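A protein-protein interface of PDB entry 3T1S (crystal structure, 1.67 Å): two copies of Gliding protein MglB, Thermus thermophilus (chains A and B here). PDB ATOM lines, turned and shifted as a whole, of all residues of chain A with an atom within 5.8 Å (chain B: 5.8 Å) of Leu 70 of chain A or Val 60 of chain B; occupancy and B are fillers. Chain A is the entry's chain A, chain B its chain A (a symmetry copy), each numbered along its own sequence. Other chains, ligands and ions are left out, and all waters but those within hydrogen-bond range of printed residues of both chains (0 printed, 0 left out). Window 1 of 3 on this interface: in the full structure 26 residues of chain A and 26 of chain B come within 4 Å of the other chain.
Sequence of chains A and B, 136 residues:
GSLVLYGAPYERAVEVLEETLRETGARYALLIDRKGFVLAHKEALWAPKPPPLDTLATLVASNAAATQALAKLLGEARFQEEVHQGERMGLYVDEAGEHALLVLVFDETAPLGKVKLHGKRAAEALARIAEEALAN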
ATOM      1  N   ALA A  66       0.934  26.584  11.341  1.00  0.00           N
ATOM      2  CA  ALA A  66       2.338  26.088  11.280  1.00  0.00           C
ATOM      3  C   ALA A  66       3.040  26.095  12.663  1.00  0.00           C
ATOM      4  O   ALA A  66       3.689  25.064  13.045  1.00  0.00           O
ATOM      5  CB  ALA A  66       3.127  26.763  10.216  1.00  0.00           C
ATOM      6  N   THR A  67       2.810  27.154  13.473  1.00  0.00           N
ATOM      7  CA  THR A  67       3.420  27.301  14.765  1.00  0.00           C
ATOM      8  C   THR A  67       2.925  26.374  15.864  1.00  0.00           C
ATOM      9  O   THR A  67       3.542  26.308  16.898  1.00  0.00           O
ATOM     10  CB  THR A  67       3.372  28.762  15.373  1.00  0.00           C
ATOM     11  OG1 THR A  67       2.063  29.094  15.833  1.00  0.00           O
ATOM     12  CG2 THR A  67       3.777  29.789  14.362  1.00  0.00           C
ATOM     13  N   GLN A  68       1.787  25.716  15.676  1.00  0.00           N
ATOM     14  CA  GLN A  68       1.304  24.780  16.717  1.00  0.00           C
ATOM     15  C   GLN A  68       2.332  23.676  17.042  1.00  0.00           C
ATOM     16  O   GLN A  68       2.477  23.321  18.216  1.00  0.00           O
ATOM     17  CB  GLN A  68      -0.103  24.224  16.387  1.00  0.00           C
ATOM     18  N   ALA A  69       3.081  23.219  16.024  1.00  0.00           N
ATOM     19  CA  ALA A  69       4.128  22.190  16.178  1.00  0.00           C
ATOM     20  C   ALA A  69       5.174  22.620  17.185  1.00  0.00           C
ATOM     21  O   ALA A  69       5.508  21.875  18.099  1.00  0.00           O
ATOM     22  CB  ALA A  69       4.756  21.796  14.838  1.00  0.00           C
ATOM     23  N   LEU A  70       5.557  23.908  17.116  1.00  0.00           N
ATOM     24  CA  LEU A  70       6.455  24.484  18.083  1.00  0.00           C
ATOM     25  C   LEU A  70       5.863  24.569  19.462  1.00  0.00           C
ATOM     26  O   LEU A  70       6.524  24.217  20.419  1.00  0.00           O
ATOM     27  CB  LEU A  70       6.897  25.928  17.650  1.00  0.00           C
ATOM     28  CG  LEU A  70       8.116  25.978  16.778  1.00  0.00           C
ATOM     29  CD1 LEU A  70       8.181  27.339  16.086  1.00  0.00           C
ATOM     30  CD2 LEU A  70       9.394  25.736  17.624  1.00  0.00           C
ATOM     31  N   ALA A  71       4.592  25.040  19.582  1.00  0.00           N
ATOM     32  CA  ALA A  71       4.021  25.159  20.905  1.00  0.00           C
ATOM     33  C   ALA A  71       3.996  23.758  21.543  1.00  0.00           C
ATOM     34  O   ALA A  71       4.299  23.637  22.725  1.00  0.00           O
ATOM     35  CB  ALA A  71       2.586  25.746  20.835  1.00  0.00           C
ATOM     36  N   LYS A  72       3.636  22.768  20.741  1.00  0.00           N
ATOM     37  CA  LYS A  72       3.474  21.365  21.235  1.00  0.00           C
ATOM     38  C   LYS A  72       4.845  20.804  21.601  1.00  0.00           C
ATOM     39  O   LYS A  72       4.964  20.150  22.664  1.00  0.00           O
ATOM     40  CB  LYS A  72       2.816  20.469  20.213  1.00  0.00           C
ATOM     41  CG  LYS A  72       1.262  20.613  20.073  1.00  0.00           C
ATOM     42  CD  LYS A  72       0.847  19.773  18.820  1.00  0.00           C
ATOM     43  CE  LYS A  72      -0.635  19.418  18.780  1.00  0.00           C
ATOM     44  NZ  LYS A  72      -1.401  20.652  18.543  1.00  0.00           N
ATOM     45  N   LEU A  73       5.866  21.060  20.758  1.00  0.00           N
ATOM     46  CA  LEU A  73       7.265  20.712  21.110  1.00  0.00           C
ATOM     47  C   LEU A  73       7.656  21.250  22.463  1.00  0.00           C
ATOM     48  O   LEU A  73       8.414  20.588  23.172  1.00  0.00           O
ATOM     49  CB  LEU A  73       8.337  21.213  20.102  1.00  0.00           C
ATOM     50  CG  LEU A  73       9.199  20.284  19.249  1.00  0.00           C
ATOM     51  CD1 LEU A  73      10.475  20.968  18.800  1.00  0.00           C
ATOM     52  CD2 LEU A  73       9.457  18.874  19.869  1.00  0.00           C
ATOM     53  N   LEU A  74       7.208  22.480  22.780  1.00  0.00           N
ATOM     54  CA  LEU A  74       7.493  23.113  24.049  1.00  0.00           C
ATOM     55  C   LEU A  74       6.500  22.818  25.147  1.00  0.00           C
ATOM     56  O   LEU A  74       6.458  23.543  26.179  1.00  0.00           O
ATOM     57  CB  LEU A  74       7.488  24.616  23.907  1.00  0.00           C
ATOM     58  CG  LEU A  74       8.473  25.263  22.935  1.00  0.00           C
ATOM     59  CD1 LEU A  74       8.241  26.732  23.041  1.00  0.00           C
ATOM     60  CD2 LEU A  74       9.923  24.919  23.279  1.00  0.00           C
ATOM     61  N   GLY A  75       5.674  21.799  24.927  1.00  0.00           N
ATOM     62  CA  GLY A  75       4.677  21.380  25.910  1.00  0.00           C
ATOM     63  C   GLY A  75       3.475  22.278  26.172  1.00  0.00           C
ATOM     64  O   GLY A  75       3.041  22.372  27.323  1.00  0.00           O
ATOM     65  N   PHE A  79       0.055  28.466  20.671  1.00  0.00           N
ATOM     66  CA  PHE A  79       0.361  29.799  21.224  1.00  0.00           C
ATOM     67  C   PHE A  79      -0.941  30.638  21.242  1.00  0.00           C
ATOM     68  O   PHE A  79      -1.875  30.354  20.452  1.00  0.00           O
ATOM     69  CB  PHE A  79       1.390  30.464  20.298  1.00  0.00           C
ATOM     70  CG  PHE A  79       2.730  29.807  20.362  1.00  0.00           C
ATOM     71  CD1 PHE A  79       3.406  29.756  21.574  1.00  0.00           C
ATOM     72  CD2 PHE A  79       3.302  29.310  19.247  1.00  0.00           C
ATOM     73  CE1 PHE A  79       4.699  29.122  21.652  1.00  0.00           C
ATOM     74  CE2 PHE A  79       4.639  28.725  19.280  1.00  0.00           C
ATOM     75  CZ  PHE A  79       5.268  28.653  20.541  1.00  0.00           C
ATOM     76  N   ILE B  32      21.370  29.452  16.494  1.00  0.00           N
ATOM     77  CA  ILE B  32      21.159  28.469  15.438  1.00  0.00           C
ATOM     78  C   ILE B  32      21.420  29.208  14.136  1.00  0.00           C
ATOM     79  O   ILE B  32      21.293  30.408  14.071  1.00  0.00           O
ATOM     80  CB  ILE B  32      19.720  27.881  15.513  1.00  0.00           C
ATOM     81  CG1 ILE B  32      18.706  28.935  15.146  1.00  0.00           C
ATOM     82  CG2 ILE B  32      19.488  27.270  16.971  1.00  0.00           C
ATOM     83  CD1 ILE B  32      17.230  28.329  14.906  1.00  0.00           C
ATOM     84  N   THR B  55      15.335  19.256  16.527  1.00  0.00           N
ATOM     85  CA  THR B  55      13.932  19.531  16.143  1.00  0.00           C
ATOM     86  C   THR B  55      13.489  20.950  16.421  1.00  0.00           C
ATOM     87  O   THR B  55      12.885  21.627  15.545  1.00  0.00           O
ATOM     88  CB  THR B  55      12.951  18.528  16.817  1.00  0.00           C
ATOM     89  OG1 THR B  55      13.558  17.236  16.731  1.00  0.00           O
ATOM     90  CG2 THR B  55      11.610  18.554  16.093  1.00  0.00           C
ATOM     91  N   LEU B  56      13.700  21.388  17.658  1.00  0.00           N
ATOM     92  CA  LEU B  56      13.356  22.773  18.005  1.00  0.00           C
ATOM     93  C   LEU B  56      14.036  23.750  17.024  1.00  0.00           C
ATOM     94  O   LEU B  56      13.350  24.579  16.405  1.00  0.00           O
ATOM     95  CB  LEU B  56      13.744  23.042  19.453  1.00  0.00           C
ATOM     96  CG  LEU B  56      13.592  24.524  19.862  1.00  0.00           C
ATOM     97  CD1 LEU B  56      12.084  24.839  19.719  1.00  0.00           C
ATOM     98  CD2 LEU B  56      14.064  24.800  21.262  1.00  0.00           C
ATOM     99  N   ALA B  57      15.345  23.628  16.828  1.00  0.00           N
ATOM    100  CA  ALA B  57      16.003  24.541  15.930  1.00  0.00           C
ATOM    101  C   ALA B  57      15.518  24.455  14.490  1.00  0.00           C
ATOM    102  O   ALA B  57      15.372  25.520  13.857  1.00  0.00           O
ATOM    103  CB  ALA B  57      17.531  24.335  15.962  1.00  0.00           C
ATOM    104  N   THR B  58      15.266  23.255  13.955  1.00  0.00           N
ATOM    105  CA  THR B  58      14.780  23.170  12.587  1.00  0.00           C
ATOM    106  C   THR B  58      13.360  23.772  12.424  1.00  0.00           C
ATOM    107  O   THR B  58      13.116  24.441  11.406  1.00  0.00           O
ATOM    108  CB  THR B  58      14.728  21.718  12.022  1.00  0.00           C
ATOM    109  OG1 THR B  58      13.925  20.931  12.853  1.00  0.00           O
ATOM    110  CG2 THR B  58      16.035  21.115  12.094  1.00  0.00           C
ATOM    111  N   LEU B  59      12.487  23.609  13.413  1.00  0.00           N
ATOM    112  CA  LEU B  59      11.111  24.221  13.375  1.00  0.00           C
ATOM    113  C   LEU B  59      11.233  25.736  13.511  1.00  0.00           C
ATOM    114  O   LEU B  59      10.603  26.448  12.740  1.00  0.00           O
ATOM    115  CB  LEU B  59      10.216  23.717  14.538  1.00  0.00           C
ATOM    116  CG  LEU B  59       9.767  22.225  14.450  1.00  0.00           C
ATOM    117  CD1 LEU B  59       8.940  21.771  15.632  1.00  0.00           C
ATOM    118  CD2 LEU B  59       9.076  21.971  13.088  1.00  0.00           C
ATOM    119  N   VAL B  60      12.114  26.233  14.426  1.00  0.00           N
ATOM    120  CA  VAL B  60      12.289  27.703  14.555  1.00  0.00           C
ATOM    121  C   VAL B  60      12.795  28.248  13.205  1.00  0.00           C
ATOM    122  O   VAL B  60      12.268  29.257  12.706  1.00  0.00           O
ATOM    123  CB  VAL B  60      13.253  28.084  15.701  1.00  0.00           C
ATOM    124  CG1 VAL B  60      13.692  29.585  15.584  1.00  0.00           C
ATOM    125  CG2 VAL B  60      12.615  27.794  17.102  1.00  0.00           C
ATOM    126  N   ALA B  61      13.793  27.593  12.589  1.00  0.00           N
ATOM    127  CA  ALA B  61      14.357  28.070  11.345  1.00  0.00           C
ATOM    128  C   ALA B  61      13.368  27.973  10.201  1.00  0.00           C
ATOM    129  O   ALA B  61      13.268  28.908   9.437  1.00  0.00           O
ATOM    130  CB  ALA B  61      15.685  27.371  11.005  1.00  0.00           C
ATOM    131  N   SER B  62      12.609  26.880  10.138  1.00  0.00           N
ATOM    132  CA  SER B  62      11.534  26.787   9.135  1.00  0.00           C
ATOM    133  C   SER B  62      10.490  27.877   9.217  1.00  0.00           C
ATOM    134  O   SER B  62      10.095  28.447   8.156  1.00  0.00           O
ATOM    135  CB  SER B  62      10.820  25.463   9.283  1.00  0.00           C
ATOM    136  OG  SER B  62      11.682  24.570   8.699  1.00  0.00           O
ATOM    137  N   ASN B  63      10.033  28.145  10.439  1.00  0.00           N
ATOM    138  CA  ASN B  63       9.058  29.216  10.667  1.00  0.00           C
ATOM    139  C   ASN B  63       9.592  30.583  10.330  1.00  0.00           C
ATOM    140  O   ASN B  63       8.883  31.455   9.748  1.00  0.00           O
ATOM    141  CB  ASN B  63       8.623  29.193  12.132  1.00  0.00           C
ATOM    142  CG  ASN B  63       7.842  30.443  12.528  1.00  0.00           C
ATOM    143  OD1 ASN B  63       8.386  31.380  13.148  1.00  0.00           O
ATOM    144  ND2 ASN B  63       6.593  30.488  12.122  1.00  0.00           N
ATOM    145  N   ALA B  64      10.873  30.800  10.646  1.00  0.00           N
ATOM    146  CA  ALA B  64      11.495  32.088  10.347  1.00  0.00           C
ATOM    147  C   ALA B  64      11.553  32.314   8.855  1.00  0.00           C
ATOM    148  O   ALA B  64      11.211  33.395   8.383  1.00  0.00           O
ATOM    149  CB  ALA B  64      12.895  32.205  10.997  1.00  0.00           C
ATOM    150  N   ALA B  65      11.872  31.271   8.089  1.00  0.00           N
ATOM    151  CA  ALA B  65      11.823  31.362   6.637  1.00  0.00           C
ATOM    152  C   ALA B  65      10.418  31.560   6.150  1.00  0.00           C
ATOM    153  O   ALA B  65      10.212  32.469   5.311  1.00  0.00           O
ATOM    154  CB  ALA B  65      12.409  30.124   6.017  1.00  0.00           C
ATOM    155  N   GLU B  82      10.753  38.003  16.732  1.00  0.00           N
ATOM    156  CA  GLU B  82       9.372  37.503  16.928  1.00  0.00           C
ATOM    157  C   GLU B  82       9.231  36.903  18.304  1.00  0.00           C
ATOM    158  O   GLU B  82      10.209  36.413  18.869  1.00  0.00           O
ATOM    159  CB  GLU B  82       8.925  36.424  15.918  1.00  0.00           C
ATOM    160  CG  GLU B  82       9.839  35.277  15.885  1.00  0.00           C
ATOM    161  CD  GLU B  82       9.515  34.377  14.733  1.00  0.00           C
ATOM    162  OE1 GLU B  82      10.452  33.969  14.031  1.00  0.00           O
ATOM    163  OE2 GLU B  82       8.339  34.111  14.477  1.00  0.00           O
ATOM    164  N   LEU B  91       8.371  31.934  23.395  1.00  0.00           N
ATOM    165  CA  LEU B  91       9.505  31.669  22.511  1.00  0.00           C
ATOM    166  C   LEU B  91       9.852  33.031  21.944  1.00  0.00           C
ATOM    167  O   LEU B  91       8.949  33.702  21.392  1.00  0.00           O
ATOM    168  CB  LEU B  91       9.067  30.766  21.405  1.00  0.00           C
ATOM    169  CG  LEU B  91      10.046  30.554  20.240  1.00  0.00           C
ATOM    170  CD1 LEU B  91      11.309  29.819  20.790  1.00  0.00           C
ATOM    171  CD2 LEU B  91       9.375  29.741  19.138  1.00  0.00           C
ATOM    172  N   VAL B  93      12.645  34.960  19.315  1.00  0.00           N
ATOM    173  CA  VAL B  93      13.673  34.732  18.359  1.00  0.00           C
ATOM    174  C   VAL B  93      14.113  36.093  17.820  1.00  0.00           C
ATOM    175  O   VAL B  93      13.297  36.942  17.462  1.00  0.00           O
ATOM    176  CB  VAL B  93      13.157  33.874  17.169  1.00  0.00           C
ATOM    177  CG1 VAL B  93      14.287  33.611  16.188  1.00  0.00           C
ATOM    178  CG2 VAL B  93      12.492  32.550  17.670  1.00  0.00           C
ATOM    179  N   LEU B 101      20.327  32.973  14.335  1.00  0.00           N
ATOM    180  CA  LEU B 101      19.176  33.443  15.126  1.00  0.00           C
ATOM    181  C   LEU B 101      19.411  33.106  16.574  1.00  0.00           C
ATOM    182  O   LEU B 101      19.945  32.004  16.843  1.00  0.00           O
ATOM    183  CB  LEU B 101      17.914  32.701  14.676  1.00  0.00           C
ATOM    184  CG  LEU B 101      17.552  32.862  13.176  1.00  0.00           C
ATOM    185  CD1 LEU B 101      16.463  31.858  12.881  1.00  0.00           C
ATOM    186  CD2 LEU B 101      16.986  34.207  13.050  1.00  0.00           C
ATOM    187  N   VAL B 103      17.639  32.137  20.008  1.00  0.00           N
ATOM    188  CA  VAL B 103      16.342  31.627  20.414  1.00  0.00           C
ATOM    189  C   VAL B 103      16.312  31.546  21.955  1.00  0.00           C
ATOM    190  O   VAL B 103      17.243  30.997  22.531  1.00  0.00           O
ATOM    191  CB  VAL B 103      16.120  30.216  19.876  1.00  0.00           C
ATOM    192  CG1 VAL B 103      14.786  29.601  20.395  1.00  0.00           C
ATOM    193  CG2 VAL B 103      16.272  30.196  18.355  1.00  0.00           C
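The backbone carbonyl oxygen of Thr 55 of chain B lies within hydrogen-bond range of the side-chain hydroxyl of Thr 58 of chain B (3.0 Å).
OE2 of Glu 82 of chain B lies close to OD1 of Asn 63 of chain B, 3.0 Å away.
Thr 67 of chain A touches Asn 63 of chain B (CG2 to ND2, 3.7 Å).
Leu 70 of chain A touches Leu 56 of chain B.
CD2 of Leu 70 of chain A touches CB of Leu 59 of chain B, 3.8 Å away.
Leu 70 of chain A touches Val 60 of chain B (CD2 to CG2, 3.9 Å).
Thr 55 of chain B touches Leu 73 of chain A.
CD1 of Leu 73 of chain A touches N of Leu 56 of chain B, at 3.4 Å.
CD1 of Leu 73 of chain A touches CD1 of Leu 59 of chain B, at 3.6 Å.
Of the printed residues of chain A, Leu 59 of chain B touches Leu 70 (3.8 Å) and Leu 73 (3.6 Å).
Of the printed residues of chain A, Val 60 of chain B touches Leu 70.
Printed residues of chain A within 4 Å of Asn 63 of chain B: Thr 67 (3.7 Å).
The nearest printed residue of chain B that does not touch Leu 70 of chain A is Leu 91 of chain B (4.1 Å).
The nearest printed residue of chain A that does not touch Val 60 of chain B is Leu 73 of chain A (7.0 Å).
The nearest printed residue of chain A that does not touch Asn 63 of chain B is Leu 70 of chain A (4.4 Å).
Hydrophobic or aromatic side chains of chain B that line the printed part of chain A: Leu 56, Leu 59 and Val 60.
Along chain B the printed residues that touch a printed residue of chain A span positions 55 to 63.
Printed residues of chain A that touch a printed residue of chain B: Thr 67, Leu 70 and Leu 73.
Hydrophobic or aromatic side chains of chain A within 4 Å of the printed part of chain B: Leu 70 and Leu 73.
Among the printed residues, 7 pairs touch across the chains.
No position is printed for both chains.
Of the 7 pairs that touch across the chains among the printed residues, none has its exchanged pair printed and touching as well.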
